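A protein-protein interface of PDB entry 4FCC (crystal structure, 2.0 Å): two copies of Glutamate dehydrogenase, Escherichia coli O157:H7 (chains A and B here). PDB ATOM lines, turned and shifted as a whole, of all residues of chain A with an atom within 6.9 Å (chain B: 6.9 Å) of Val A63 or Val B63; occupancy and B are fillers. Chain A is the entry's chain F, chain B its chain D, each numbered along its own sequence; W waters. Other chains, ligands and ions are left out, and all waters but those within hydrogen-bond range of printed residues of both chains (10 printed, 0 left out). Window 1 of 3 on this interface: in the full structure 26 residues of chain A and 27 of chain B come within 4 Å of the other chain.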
ATOM      1  N   PRO A  60     -12.691   6.630 -13.178  1.00  0.00           N
ATOM      2  CA  PRO A  60     -13.746   7.378 -13.874  1.00  0.00           C
ATOM      3  C   PRO A  60     -13.198   8.669 -14.471  1.00  0.00           C
ATOM      4  O   PRO A  60     -12.318   9.291 -13.891  1.00  0.00           O
ATOM      5  CB  PRO A  60     -14.752   7.691 -12.761  1.00  0.00           C
ATOM      6  CG  PRO A  60     -13.927   7.683 -11.500  1.00  0.00           C
ATOM      7  CD  PRO A  60     -12.906   6.594 -11.720  1.00  0.00           C
ATOM      8  N   GLU A  61     -13.708   9.054 -15.632  1.00  0.00           N
ATOM      9  CA  GLU A  61     -13.231  10.253 -16.315  1.00  0.00           C
ATOM     10  C   GLU A  61     -13.402  11.486 -15.446  1.00  0.00           C
ATOM     11  O   GLU A  61     -12.484  12.306 -15.311  1.00  0.00           O
ATOM     12  CB  GLU A  61     -13.923  10.401 -17.668  1.00  0.00           C
ATOM     13  CG  GLU A  61     -13.551   9.256 -18.603  1.00  0.00           C
ATOM     14  CD  GLU A  61     -14.268   9.296 -19.943  1.00  0.00           C
ATOM     15  OE1 GLU A  61     -14.826  10.356 -20.301  1.00  0.00           O
ATOM     16  OE2 GLU A  61     -14.278   8.255 -20.632  1.00  0.00           O
ATOM     17  N   ARG A  62     -14.567  11.601 -14.821  1.00  0.00           N
ATOM     18  CA  ARG A  62     -14.766  12.658 -13.842  1.00  0.00           C
ATOM     19  C   ARG A  62     -15.945  12.383 -12.918  1.00  0.00           C
ATOM     20  O   ARG A  62     -16.926  11.742 -13.305  1.00  0.00           O
ATOM     21  CB  ARG A  62     -14.918  14.030 -14.516  1.00  0.00           C
ATOM     22  CG  ARG A  62     -16.323  14.379 -14.954  1.00  0.00           C
ATOM     23  CD  ARG A  62     -16.429  15.849 -15.378  1.00  0.00           C
ATOM     24  NE  ARG A  62     -15.608  16.145 -16.553  1.00  0.00           N
ATOM     25  CZ  ARG A  62     -15.996  15.934 -17.806  1.00  0.00           C
ATOM     26  NH1 ARG A  62     -17.197  15.419 -18.044  1.00  0.00           N
ATOM     27  NH2 ARG A  62     -15.186  16.239 -18.824  1.00  0.00           N
ATOM     28  N   VAL A  63     -15.826  12.881 -11.693  1.00  0.00           N
ATOM     29  CA  VAL A  63     -16.895  12.802 -10.718  1.00  0.00           C
ATOM     30  C   VAL A  63     -17.172  14.209 -10.223  1.00  0.00           C
ATOM     31  O   VAL A  63     -16.252  14.926  -9.831  1.00  0.00           O
ATOM     32  CB  VAL A  63     -16.480  11.953  -9.484  1.00  0.00           C
ATOM     33  CG1 VAL A  63     -17.567  11.993  -8.436  1.00  0.00           C
ATOM     34  CG2 VAL A  63     -16.158  10.522  -9.887  1.00  0.00           C
ATOM     35  N   ILE A  64     -18.433  14.611 -10.234  1.00  0.00           N
ATOM     36  CA  ILE A  64     -18.790  15.863  -9.603  1.00  0.00           C
ATOM     37  C   ILE A  64     -19.502  15.563  -8.302  1.00  0.00           C
ATOM     38  O   ILE A  64     -20.563  14.952  -8.311  1.00  0.00           O
ATOM     39  CB  ILE A  64     -19.727  16.717 -10.469  1.00  0.00           C
ATOM     40  CG1 ILE A  64     -19.151  16.895 -11.885  1.00  0.00           C
ATOM     41  CG2 ILE A  64     -19.960  18.084  -9.805  1.00  0.00           C
ATOM     42  CD1 ILE A  64     -19.949  16.177 -12.938  1.00  0.00           C
ATOM     43  N   GLN A  65     -18.901  15.967  -7.190  1.00  0.00           N
ATOM     44  CA  GLN A  65     -19.596  15.949  -5.904  1.00  0.00           C
ATOM     45  C   GLN A  65     -20.007  17.379  -5.627  1.00  0.00           C
ATOM     46  O   GLN A  65     -19.210  18.310  -5.807  1.00  0.00           O
ATOM     47  CB  GLN A  65     -18.696  15.438  -4.769  1.00  0.00           C
ATOM     48  CG  GLN A  65     -19.365  15.500  -3.386  1.00  0.00           C
ATOM     49  CD  GLN A  65     -18.367  15.456  -2.227  1.00  0.00           C
ATOM     50  OE1 GLN A  65     -17.819  14.405  -1.908  1.00  0.00           O
ATOM     51  NE2 GLN A  65     -18.143  16.607  -1.587  1.00  0.00           N
ATOM     52  N   PHE A  66     -21.253  17.565  -5.217  1.00  0.00           N
ATOM     53  CA  PHE A  66     -21.724  18.903  -4.920  1.00  0.00           C
ATOM     54  C   PHE A  66     -22.738  19.004  -3.789  1.00  0.00           C
ATOM     55  O   PHE A  66     -23.509  18.069  -3.518  1.00  0.00           O
ATOM     56  CB  PHE A  66     -22.277  19.586  -6.161  1.00  0.00           C
ATOM     57  CG  PHE A  66     -23.418  18.858  -6.818  1.00  0.00           C
ATOM     58  CD1 PHE A  66     -23.188  17.740  -7.607  1.00  0.00           C
ATOM     59  CD2 PHE A  66     -24.714  19.325  -6.695  1.00  0.00           C
ATOM     60  CE1 PHE A  66     -24.237  17.080  -8.226  1.00  0.00           C
ATOM     61  CE2 PHE A  66     -25.758  18.672  -7.329  1.00  0.00           C
ATOM     62  CZ  PHE A  66     -25.512  17.547  -8.101  1.00  0.00           C
ATOM     63  N   ARG A  67     -22.729  20.171  -3.152  1.00  0.00           N
ATOM     64  CA  ARG A  67     -23.669  20.499  -2.094  1.00  0.00           C
ATOM     65  C   ARG A  67     -25.051  20.767  -2.685  1.00  0.00           C
ATOM     66  O   ARG A  67     -25.169  21.380  -3.747  1.00  0.00           O
ATOM     67  CB  ARG A  67     -23.166  21.736  -1.346  1.00  0.00           C
ATOM     68  CG  ARG A  67     -23.997  22.175  -0.165  1.00  0.00           C
ATOM     69  CD  ARG A  67     -23.405  23.403   0.478  1.00  0.00           C
ATOM     70  NE  ARG A  67     -23.567  24.608  -0.336  1.00  0.00           N
ATOM     71  CZ  ARG A  67     -23.007  25.785  -0.052  1.00  0.00           C
ATOM     72  NH1 ARG A  67     -22.231  25.930   1.025  1.00  0.00           N
ATOM     73  NH2 ARG A  67     -23.223  26.823  -0.847  1.00  0.00           N
ATOM     74  N   TRP A  83     -23.985  13.657  -6.256  1.00  0.00           N
ATOM     75  CA  TRP A  83     -22.871  13.348  -7.131  1.00  0.00           C
ATOM     76  C   TRP A  83     -23.366  13.103  -8.537  1.00  0.00           C
ATOM     77  O   TRP A  83     -24.518  12.727  -8.740  1.00  0.00           O
ATOM     78  CB  TRP A  83     -22.195  12.042  -6.745  1.00  0.00           C
ATOM     79  CG  TRP A  83     -21.608  11.908  -5.408  1.00  0.00           C
ATOM     80  CD1 TRP A  83     -20.282  11.955  -5.089  1.00  0.00           C
ATOM     81  CD2 TRP A  83     -22.306  11.608  -4.200  1.00  0.00           C
ATOM     82  NE1 TRP A  83     -20.116  11.734  -3.739  1.00  0.00           N
ATOM     83  CE2 TRP A  83     -21.346  11.512  -3.175  1.00  0.00           C
ATOM     84  CE3 TRP A  83     -23.653  11.414  -3.883  1.00  0.00           C
ATOM     85  CZ2 TRP A  83     -21.690  11.229  -1.857  1.00  0.00           C
ATOM     86  CZ3 TRP A  83     -23.992  11.141  -2.562  1.00  0.00           C
ATOM     87  CH2 TRP A  83     -23.015  11.063  -1.573  1.00  0.00           C
ATOM     88  N   ARG A  84     -22.467  13.267  -9.501  1.00  0.00           N
ATOM     89  CA  ARG A  84     -22.638  12.625 -10.795  1.00  0.00           C
ATOM     90  C   ARG A  84     -21.307  12.015 -11.216  1.00  0.00           C
ATOM     91  O   ARG A  84     -20.311  12.715 -11.435  1.00  0.00           O
ATOM     92  CB  ARG A  84     -23.169  13.589 -11.861  1.00  0.00           C
ATOM     93  CG  ARG A  84     -23.392  12.933 -13.220  1.00  0.00           C
ATOM     94  CD  ARG A  84     -24.588  11.979 -13.201  1.00  0.00           C
ATOM     95  NE  ARG A  84     -24.893  11.419 -14.522  1.00  0.00           N
ATOM     96  CZ  ARG A  84     -25.714  10.387 -14.727  1.00  0.00           C
ATOM     97  NH1 ARG A  84     -26.326   9.799 -13.695  1.00  0.00           N
ATOM     98  NH2 ARG A  84     -25.935   9.950 -15.965  1.00  0.00           N
ATOM     99  N   VAL A  85     -21.293  10.693 -11.303  1.00  0.00           N
ATOM    100  CA  VAL A  85     -20.118   9.978 -11.718  1.00  0.00           C
ATOM    101  C   VAL A  85     -20.213   9.825 -13.213  1.00  0.00           C
ATOM    102  O   VAL A  85     -21.110   9.163 -13.721  1.00  0.00           O
ATOM    103  CB  VAL A  85     -20.045   8.602 -11.058  1.00  0.00           C
ATOM    104  CG1 VAL A  85     -18.772   7.902 -11.464  1.00  0.00           C
ATOM    105  CG2 VAL A  85     -20.131   8.761  -9.535  1.00  0.00           C
ATOM    106  N   GLN A  86     -19.307  10.483 -13.922  1.00  0.00           N
ATOM    107  CA  GLN A  86     -19.284  10.381 -15.364  1.00  0.00           C
ATOM    108  C   GLN A  86     -18.139   9.430 -15.663  1.00  0.00           C
ATOM    109  O   GLN A  86     -16.991   9.834 -15.788  1.00  0.00           O
ATOM    110  CB  GLN A  86     -19.117  11.776 -15.986  1.00  0.00           C
ATOM    111  CG  GLN A  86     -20.283  12.697 -15.595  1.00  0.00           C
ATOM    112  CD  GLN A  86     -20.249  14.066 -16.238  1.00  0.00           C
ATOM    113  OE1 GLN A  86     -19.186  14.610 -16.534  1.00  0.00           O
ATOM    114  NE2 GLN A  86     -21.423  14.637 -16.445  1.00  0.00           N
ATOM    115  N   PHE A  87     -18.460   8.142 -15.717  1.00  0.00           N
ATOM    116  CA  PHE A  87     -17.417   7.131 -15.699  1.00  0.00           C
ATOM    117  C   PHE A  87     -16.712   7.016 -17.036  1.00  0.00           C
ATOM    118  O   PHE A  87     -15.483   7.141 -17.110  1.00  0.00           O
ATOM    119  CB  PHE A  87     -17.973   5.771 -15.252  1.00  0.00           C
ATOM    120  CG  PHE A  87     -17.011   4.977 -14.416  1.00  0.00           C
ATOM    121  CD1 PHE A  87     -15.819   4.515 -14.958  1.00  0.00           C
ATOM    122  CD2 PHE A  87     -17.287   4.713 -13.087  1.00  0.00           C
ATOM    123  CE1 PHE A  87     -14.926   3.792 -14.190  1.00  0.00           C
ATOM    124  CE2 PHE A  87     -16.400   3.983 -12.309  1.00  0.00           C
ATOM    125  CZ  PHE A  87     -15.217   3.518 -12.858  1.00  0.00           C
ATOM    126  N   LEU A 106     -20.113   7.679  -2.672  1.00  0.00           N
ATOM    127  CA  LEU A 106     -19.316   7.644  -3.892  1.00  0.00           C
ATOM    128  C   LEU A 106     -18.940   6.211  -4.277  1.00  0.00           C
ATOM    129  O   LEU A 106     -18.943   5.862  -5.453  1.00  0.00           O
ATOM    130  CB  LEU A 106     -18.075   8.521  -3.755  1.00  0.00           C
ATOM    131  CG  LEU A 106     -17.116   8.583  -4.950  1.00  0.00           C
ATOM    132  CD1 LEU A 106     -17.801   9.105  -6.212  1.00  0.00           C
ATOM    133  CD2 LEU A 106     -15.917   9.432  -4.586  1.00  0.00           C
ATOM    134  N   LYS A 110     -19.955   4.743  -7.901  1.00  0.00           N
ATOM    135  CA  LYS A 110     -18.854   4.309  -8.763  1.00  0.00           C
ATOM    136  C   LYS A 110     -19.028   2.867  -9.194  1.00  0.00           C
ATOM    137  O   LYS A 110     -18.815   2.528 -10.357  1.00  0.00           O
ATOM    138  CB  LYS A 110     -17.498   4.475  -8.070  1.00  0.00           C
ATOM    139  CG  LYS A 110     -16.961   5.905  -8.092  1.00  0.00           C
ATOM    140  CD  LYS A 110     -15.599   6.013  -7.393  1.00  0.00           C
ATOM    141  CE  LYS A 110     -14.541   5.166  -8.101  1.00  0.00           C
ATOM    142  NZ  LYS A 110     -13.180   5.280  -7.473  1.00  0.00           N
ATOM    143  N   PRO B  60     -18.503  21.442   0.852  1.00  0.00           N
ATOM    144  CA  PRO B  60     -17.943  22.230  -0.253  1.00  0.00           C
ATOM    145  C   PRO B  60     -18.958  22.417  -1.371  1.00  0.00           C
ATOM    146  O   PRO B  60     -19.734  21.509  -1.621  1.00  0.00           O
ATOM    147  CB  PRO B  60     -16.769  21.369  -0.745  1.00  0.00           C
ATOM    148  CG  PRO B  60     -17.050  19.981  -0.224  1.00  0.00           C
ATOM    149  CD  PRO B  60     -17.764  20.188   1.073  1.00  0.00           C
ATOM    150  N   GLU B  61     -18.948  23.571  -2.039  1.00  0.00           N
ATOM    151  CA  GLU B  61     -19.948  23.832  -3.063  1.00  0.00           C
ATOM    152  C   GLU B  61     -19.859  22.789  -4.189  1.00  0.00           C
ATOM    153  O   GLU B  61     -20.879  22.293  -4.704  1.00  0.00           O
ATOM    154  CB  GLU B  61     -19.811  25.273  -3.580  1.00  0.00           C
ATOM    155  CG  GLU B  61     -20.302  26.315  -2.564  1.00  0.00           C
ATOM    156  CD  GLU B  61     -19.904  27.743  -2.927  1.00  0.00           C
ATOM    157  OE1 GLU B  61     -19.590  27.999  -4.114  1.00  0.00           O
ATOM    158  OE2 GLU B  61     -19.902  28.612  -2.021  1.00  0.00           O
ATOM    159  N   ARG B  62     -18.633  22.393  -4.503  1.00  0.00           N
ATOM    160  CA  ARG B  62     -18.389  21.510  -5.627  1.00  0.00           C
ATOM    161  C   ARG B  62     -16.974  20.932  -5.552  1.00  0.00           C
ATOM    162  O   ARG B  62     -16.003  21.664  -5.348  1.00  0.00           O
ATOM    163  CB  ARG B  62     -18.581  22.316  -6.921  1.00  0.00           C
ATOM    164  CG  ARG B  62     -18.406  21.553  -8.216  1.00  0.00           C
ATOM    165  CD  ARG B  62     -18.237  22.526  -9.393  1.00  0.00           C
ATOM    166  NE  ARG B  62     -19.403  23.391  -9.571  1.00  0.00           N
ATOM    167  CZ  ARG B  62     -19.394  24.710  -9.414  1.00  0.00           C
ATOM    168  NH1 ARG B  62     -18.266  25.350  -9.097  1.00  0.00           N
ATOM    169  NH2 ARG B  62     -20.509  25.400  -9.603  1.00  0.00           N
ATOM    170  N   VAL B  63     -16.864  19.619  -5.703  1.00  0.00           N
ATOM    171  CA  VAL B  63     -15.572  18.965  -5.890  1.00  0.00           C
ATOM    172  C   VAL B  63     -15.561  18.244  -7.232  1.00  0.00           C
ATOM    173  O   VAL B  63     -16.503  17.510  -7.562  1.00  0.00           O
ATOM    174  CB  VAL B  63     -15.276  17.918  -4.804  1.00  0.00           C
ATOM    175  CG1 VAL B  63     -13.902  17.284  -5.035  1.00  0.00           C
ATOM    176  CG2 VAL B  63     -15.358  18.525  -3.418  1.00  0.00           C
ATOM    177  N   ILE B  64     -14.503  18.447  -8.006  1.00  0.00           N
ATOM    178  CA  ILE B  64     -14.309  17.685  -9.235  1.00  0.00           C
ATOM    179  C   ILE B  64     -13.113  16.754  -9.056  1.00  0.00           C
ATOM    180  O   ILE B  64     -11.998  17.214  -8.832  1.00  0.00           O
ATOM    181  CB  ILE B  64     -14.050  18.606 -10.461  1.00  0.00           C
ATOM    182  CG1 ILE B  64     -15.211  19.585 -10.659  1.00  0.00           C
ATOM    183  CG2 ILE B  64     -13.839  17.772 -11.714  1.00  0.00           C
ATOM    184  CD1 ILE B  64     -14.832  21.037 -10.396  1.00  0.00           C
ATOM    185  N   GLN B  65     -13.360  15.448  -9.120  1.00  0.00           N
ATOM    186  CA  GLN B  65     -12.300  14.452  -9.182  1.00  0.00           C
ATOM    187  C   GLN B  65     -12.243  14.006 -10.629  1.00  0.00           C
ATOM    188  O   GLN B  65     -13.281  13.820 -11.260  1.00  0.00           O
ATOM    189  CB  GLN B  65     -12.611  13.242  -8.298  1.00  0.00           C
ATOM    190  CG  GLN B  65     -11.683  12.045  -8.562  1.00  0.00           C
ATOM    191  CD  GLN B  65     -12.223  10.720  -8.032  1.00  0.00           C
ATOM    192  OE1 GLN B  65     -12.334   9.739  -8.777  1.00  0.00           O
ATOM    193  NE2 GLN B  65     -12.539  10.678  -6.735  1.00  0.00           N
ATOM    194  N   PHE B  66     -11.042  13.843 -11.168  1.00  0.00           N
ATOM    195  CA  PHE B  66     -10.933  13.442 -12.555  1.00  0.00           C
ATOM    196  C   PHE B  66      -9.676  12.655 -12.854  1.00  0.00           C
ATOM    197  O   PHE B  66      -8.679  12.748 -12.135  1.00  0.00           O
ATOM    198  CB  PHE B  66     -11.045  14.660 -13.485  1.00  0.00           C
ATOM    199  CG  PHE B  66      -9.987  15.718 -13.264  1.00  0.00           C
ATOM    200  CD1 PHE B  66     -10.169  16.712 -12.322  1.00  0.00           C
ATOM    201  CD2 PHE B  66      -8.840  15.754 -14.053  1.00  0.00           C
ATOM    202  CE1 PHE B  66      -9.214  17.708 -12.135  1.00  0.00           C
ATOM    203  CE2 PHE B  66      -7.880  16.740 -13.868  1.00  0.00           C
ATOM    204  CZ  PHE B  66      -8.068  17.716 -12.911  1.00  0.00           C
ATOM    205  N   ARG B  67      -9.745  11.885 -13.935  1.00  0.00           N
ATOM    206  CA  ARG B  67      -8.641  11.051 -14.389  1.00  0.00           C
ATOM    207  C   ARG B  67      -7.624  11.876 -15.163  1.00  0.00           C
ATOM    208  O   ARG B  67      -7.994  12.716 -15.992  1.00  0.00           O
ATOM    209  CB  ARG B  67      -9.169   9.922 -15.280  1.00  0.00           C
ATOM    210  CG  ARG B  67      -8.096   8.972 -15.797  1.00  0.00           C
ATOM    211  CD  ARG B  67      -8.694   7.897 -16.708  1.00  0.00           C
ATOM    212  NE  ARG B  67      -9.187   8.468 -17.963  1.00  0.00           N
ATOM    213  CZ  ARG B  67     -10.043   7.854 -18.780  1.00  0.00           C
ATOM    214  NH1 ARG B  67     -10.503   6.649 -18.476  1.00  0.00           N
ATOM    215  NH2 ARG B  67     -10.443   8.445 -19.902  1.00  0.00           N
ATOM    216  N   TRP B  83      -7.913  16.410  -8.490  1.00  0.00           N
ATOM    217  CA  TRP B  83      -9.093  17.021  -7.925  1.00  0.00           C
ATOM    218  C   TRP B  83      -8.960  18.531  -8.023  1.00  0.00           C
ATOM    219  O   TRP B  83      -7.854  19.068  -7.923  1.00  0.00           O
ATOM    220  CB  TRP B  83      -9.201  16.727  -6.426  1.00  0.00           C
ATOM    221  CG  TRP B  83      -9.217  15.301  -5.951  1.00  0.00           C
ATOM    222  CD1 TRP B  83     -10.313  14.581  -5.545  1.00  0.00           C
ATOM    223  CD2 TRP B  83      -8.083  14.451  -5.737  1.00  0.00           C
ATOM    224  NE1 TRP B  83      -9.928  13.326  -5.123  1.00  0.00           N
ATOM    225  CE2 TRP B  83      -8.567  13.220  -5.235  1.00  0.00           C
ATOM    226  CE3 TRP B  83      -6.710  14.599  -5.941  1.00  0.00           C
ATOM    227  CZ2 TRP B  83      -7.726  12.155  -4.931  1.00  0.00           C
ATOM    228  CZ3 TRP B  83      -5.874  13.533  -5.638  1.00  0.00           C
ATOM    229  CH2 TRP B  83      -6.387  12.330  -5.139  1.00  0.00           C
ATOM    230  N   ARG B  84     -10.091  19.209  -8.190  1.00  0.00           N
ATOM    231  CA  ARG B  84     -10.236  20.588  -7.733  1.00  0.00           C
ATOM    232  C   ARG B  84     -11.399  20.676  -6.750  1.00  0.00           C
ATOM    233  O   ARG B  84     -12.548  20.412  -7.105  1.00  0.00           O
ATOM    234  CB  ARG B  84     -10.487  21.560  -8.877  1.00  0.00           C
ATOM    235  CG  ARG B  84     -10.582  23.021  -8.411  1.00  0.00           C
ATOM    236  CD  ARG B  84      -9.239  23.499  -7.808  1.00  0.00           C
ATOM    237  NE  ARG B  84      -9.212  24.945  -7.543  1.00  0.00           N
ATOM    238  CZ  ARG B  84      -8.209  25.584  -6.943  1.00  0.00           C
ATOM    239  NH1 ARG B  84      -7.136  24.915  -6.547  1.00  0.00           N
ATOM    240  NH2 ARG B  84      -8.276  26.893  -6.734  1.00  0.00           N
ATOM    241  N   VAL B  85     -11.089  21.033  -5.510  1.00  0.00           N
ATOM    242  CA  VAL B  85     -12.115  21.257  -4.506  1.00  0.00           C
ATOM    243  C   VAL B  85     -12.517  22.719  -4.549  1.00  0.00           C
ATOM    244  O   VAL B  85     -11.724  23.599  -4.234  1.00  0.00           O
ATOM    245  CB  VAL B  85     -11.614  20.913  -3.085  1.00  0.00           C
ATOM    246  CG1 VAL B  85     -12.709  21.193  -2.067  1.00  0.00           C
ATOM    247  CG2 VAL B  85     -11.158  19.450  -3.017  1.00  0.00           C
ATOM    248  N   GLN B  86     -13.748  22.986  -4.953  1.00  0.00           N
ATOM    249  CA  GLN B  86     -14.206  24.362  -5.015  1.00  0.00           C
ATOM    250  C   GLN B  86     -15.085  24.618  -3.799  1.00  0.00           C
ATOM    251  O   GLN B  86     -16.294  24.345  -3.802  1.00  0.00           O
ATOM    252  CB  GLN B  86     -14.884  24.642  -6.361  1.00  0.00           C
ATOM    253  CG  GLN B  86     -13.903  24.430  -7.517  1.00  0.00           C
ATOM    254  CD  GLN B  86     -14.490  24.701  -8.896  1.00  0.00           C
ATOM    255  OE1 GLN B  86     -15.692  24.570  -9.115  1.00  0.00           O
ATOM    256  NE2 GLN B  86     -13.631  25.076  -9.835  1.00  0.00           N
ATOM    257  N   PHE B  87     -14.456  25.122  -2.740  1.00  0.00           N
ATOM    258  CA  PHE B  87     -15.093  25.067  -1.423  1.00  0.00           C
ATOM    259  C   PHE B  87     -16.148  26.150  -1.229  1.00  0.00           C
ATOM    260  O   PHE B  87     -17.311  25.842  -0.950  1.00  0.00           O
ATOM    261  CB  PHE B  87     -14.072  25.058  -0.271  1.00  0.00           C
ATOM    262  CG  PHE B  87     -14.489  24.172   0.891  1.00  0.00           C
ATOM    263  CD1 PHE B  87     -15.614  24.473   1.638  1.00  0.00           C
ATOM    264  CD2 PHE B  87     -13.785  23.024   1.195  1.00  0.00           C
ATOM    265  CE1 PHE B  87     -16.030  23.650   2.688  1.00  0.00           C
ATOM    266  CE2 PHE B  87     -14.179  22.205   2.238  1.00  0.00           C
ATOM    267  CZ  PHE B  87     -15.309  22.521   2.983  1.00  0.00           C
ATOM    268  N   LEU B 106      -8.565  13.369  -1.190  1.00  0.00           N
ATOM    269  CA  LEU B 106      -9.646  14.337  -1.044  1.00  0.00           C
ATOM    270  C   LEU B 106      -9.753  14.865   0.386  1.00  0.00           C
ATOM    271  O   LEU B 106     -10.128  16.021   0.599  1.00  0.00           O
ATOM    272  CB  LEU B 106     -10.979  13.741  -1.513  1.00  0.00           C
ATOM    273  CG  LEU B 106     -12.263  14.566  -1.371  1.00  0.00           C
ATOM    274  CD1 LEU B 106     -12.196  15.892  -2.139  1.00  0.00           C
ATOM    275  CD2 LEU B 106     -13.491  13.753  -1.809  1.00  0.00           C
ATOM    276  N   LYS B 110      -9.610  18.828   1.063  1.00  0.00           N
ATOM    277  CA  LYS B 110     -10.764  19.448   1.705  1.00  0.00           C
ATOM    278  C   LYS B 110     -10.322  20.224   2.945  1.00  0.00           C
ATOM    279  O   LYS B 110     -10.710  21.377   3.129  1.00  0.00           O
ATOM    280  CB  LYS B 110     -11.830  18.400   2.063  1.00  0.00           C
ATOM    281  CG  LYS B 110     -12.682  17.973   0.875  1.00  0.00           C
ATOM    282  CD  LYS B 110     -13.721  16.946   1.267  1.00  0.00           C
ATOM    283  CE  LYS B 110     -14.729  17.552   2.219  1.00  0.00           C
ATOM    284  NZ  LYS B 110     -15.669  16.520   2.730  1.00  0.00           N
HETATM  285  O   HOH W   1     -16.271  14.292   0.463  1.00  0.00           O
HETATM  286  O   HOH W   2     -10.754  13.076 -17.156  1.00  0.00           O
HETATM  287  O   HOH W   3     -12.555   6.194 -20.425  1.00  0.00           O
HETATM  288  O   HOH W   4     -12.894   5.469 -17.129  1.00  0.00           O
HETATM  289  O   HOH W   5     -13.002   7.642  -5.960  1.00  0.00           O
HETATM  290  O   HOH W   6     -20.745  28.316   0.215  1.00  0.00           O
HETATM  291  O   HOH W   7     -23.230  23.197  -4.952  1.00  0.00           O
HETATM  292  O   HOH W   8     -20.231  18.478  -1.954  1.00  0.00           O
HETATM  293  O   HOH W   9     -11.244  10.406 -11.435  1.00  0.00           O
HETATM  294  O   HOH W  10     -19.152  25.449   1.059  1.00  0.00           O
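Of the 15 printed residues of chain A, 8 touch a printed residue of chain B. Among the printed residues, 15 pairs touch across the chains. Among the printed residues, Asp or Glu carboxylates within 4 Å of a Lys or Arg side-chain nitrogen of the other chain: Glu A61 with Arg B67 (3.9 Å) and Arg A67 with Glu B61 (3.95 Å).
Water W6 lies within hydrogen-bond range of the side-chain carboxylate (OE2) of Glu B61 (2.4 Å) and the guanidinium group (NH1) of Arg A67 (2.9 Å). Water W7 bridges O of Glu B61 and O of Arg A67. Water W3 lies within hydrogen-bond range of OE2 of Glu A61 (2.7 Å) and NH1 of Arg B67 (2.9 Å). Water W10 bridges the backbone carbonyl oxygen (O) of Phe B87 (2.8 Å) and the guanidinium group (NH1) of Arg A67 (3.1 Å). Water W5 bridges the side-chain amino group of Lys A110 and the side-chain amide nitrogen of Gln B65. Water W4 lies within hydrogen-bond range of NH1 of Arg B67 (3.0 Å) and O of Phe A87 (3.1 Å).
Val B63 touches just these residues of chain A: Val A63, Ile A64 and Gln A65. Of the printed residues of chain B, Phe A66 touches Glu B61 (3.4 Å). Printed residues of chain A within 4 Å of Arg B62: Gln A65 (3.3 Å). Of the printed residues of chain A, Phe B66 touches Glu A61 (3.3 Å). Of the printed residues of chain B, Arg A62 touches Gln B65 (3.2 Å). Of the printed residues of chain B, Glu A61 touches Phe B66 (3.3 Å) and Arg B67 (3.1 Å). The nearest residue of chain B that does not touch Val A63 is Phe B66 (4.9 Å). The nearest residue of chain A that does not touch Val B63 is Phe A66 (4.9 Å). The nearest printed residue of chain A that does not touch Phe B66 is Arg A62 (4.1 Å).
Pro A60 touches Arg B67, and with the chains exchanged Arg A67 touches Pro B60. Glu A61 touches Phe B66, and with the chains exchanged Phe A66 touches Glu B61. Val A63 touches its own counterpart, Val B63. Val A63 touches Ile B64, and with the chains exchanged Ile A64 touches Val B63. Positions printed for both chains: 60, 61, 62, 63, 64, 65, 66, 67, 83, 84, 85, 86, 87, 106 and 110. Of the 15 pairs that touch across the chains among the printed residues, 15 have their exchanged pair printed and touching as well.
Among the printed residues, pairs that only touch across the chains: Arg A62 with Gln B65 (3.2 Å), Glu A61 with Phe B66 (3.3 Å), Gln A65 with Arg B62 (3.3 Å), Phe A66 with Glu B61 (3.4 Å), Val A63 with Ile B64 (3.4 Å), Arg A67 with Pro B60 (3.5 Å), Ile A64 with Val B63 (3.5 Å), Pro A60 with Arg B67 (3.5 Å), Pro A60 with Gln B65 (3.8 Å) and Gln A65 with Pro B60 (3.8 Å).
O of Phe B87 is in hydrogen-bond range of N of Glu B61, 3.0 Å away. N of Arg B84 sits at hydrogen-bond distance from O of Ile B64 (2.8 Å). The backbone carbonyl oxygen (O) of Ile A64 is in hydrogen-bond range of the backbone NH (N) of Arg A84, at 2.8 Å. The side-chain amide oxygen (OE1) of Gln A86 sits at hydrogen-bond distance from the guanidinium group (NH1) of Arg A62 (2.6 Å). O of Gln B86 sits at hydrogen-bond distance from N of Glu B61. The backbone carbonyl oxygen of Arg B62 is in hydrogen-bond range of the backbone NH of Gln B86 (2.6 Å).
O of Val B63 sits close to O of Val A63 (3.4 Å). N of Val B63 lies within hydrogen-bond range of O of Gln A65 (2.7 Å). NH2 of Arg B67 lies within salt-bridge range of OE2 of Glu A61, 3.9 Å away. N of Val A63 is in hydrogen-bond range of O of Gln B65 (2.7 Å). The guanidinium group (NH2) of Arg A67 lies within salt-bridge range of the side-chain carboxylate (OE2) of Glu B61 (3.95 Å).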
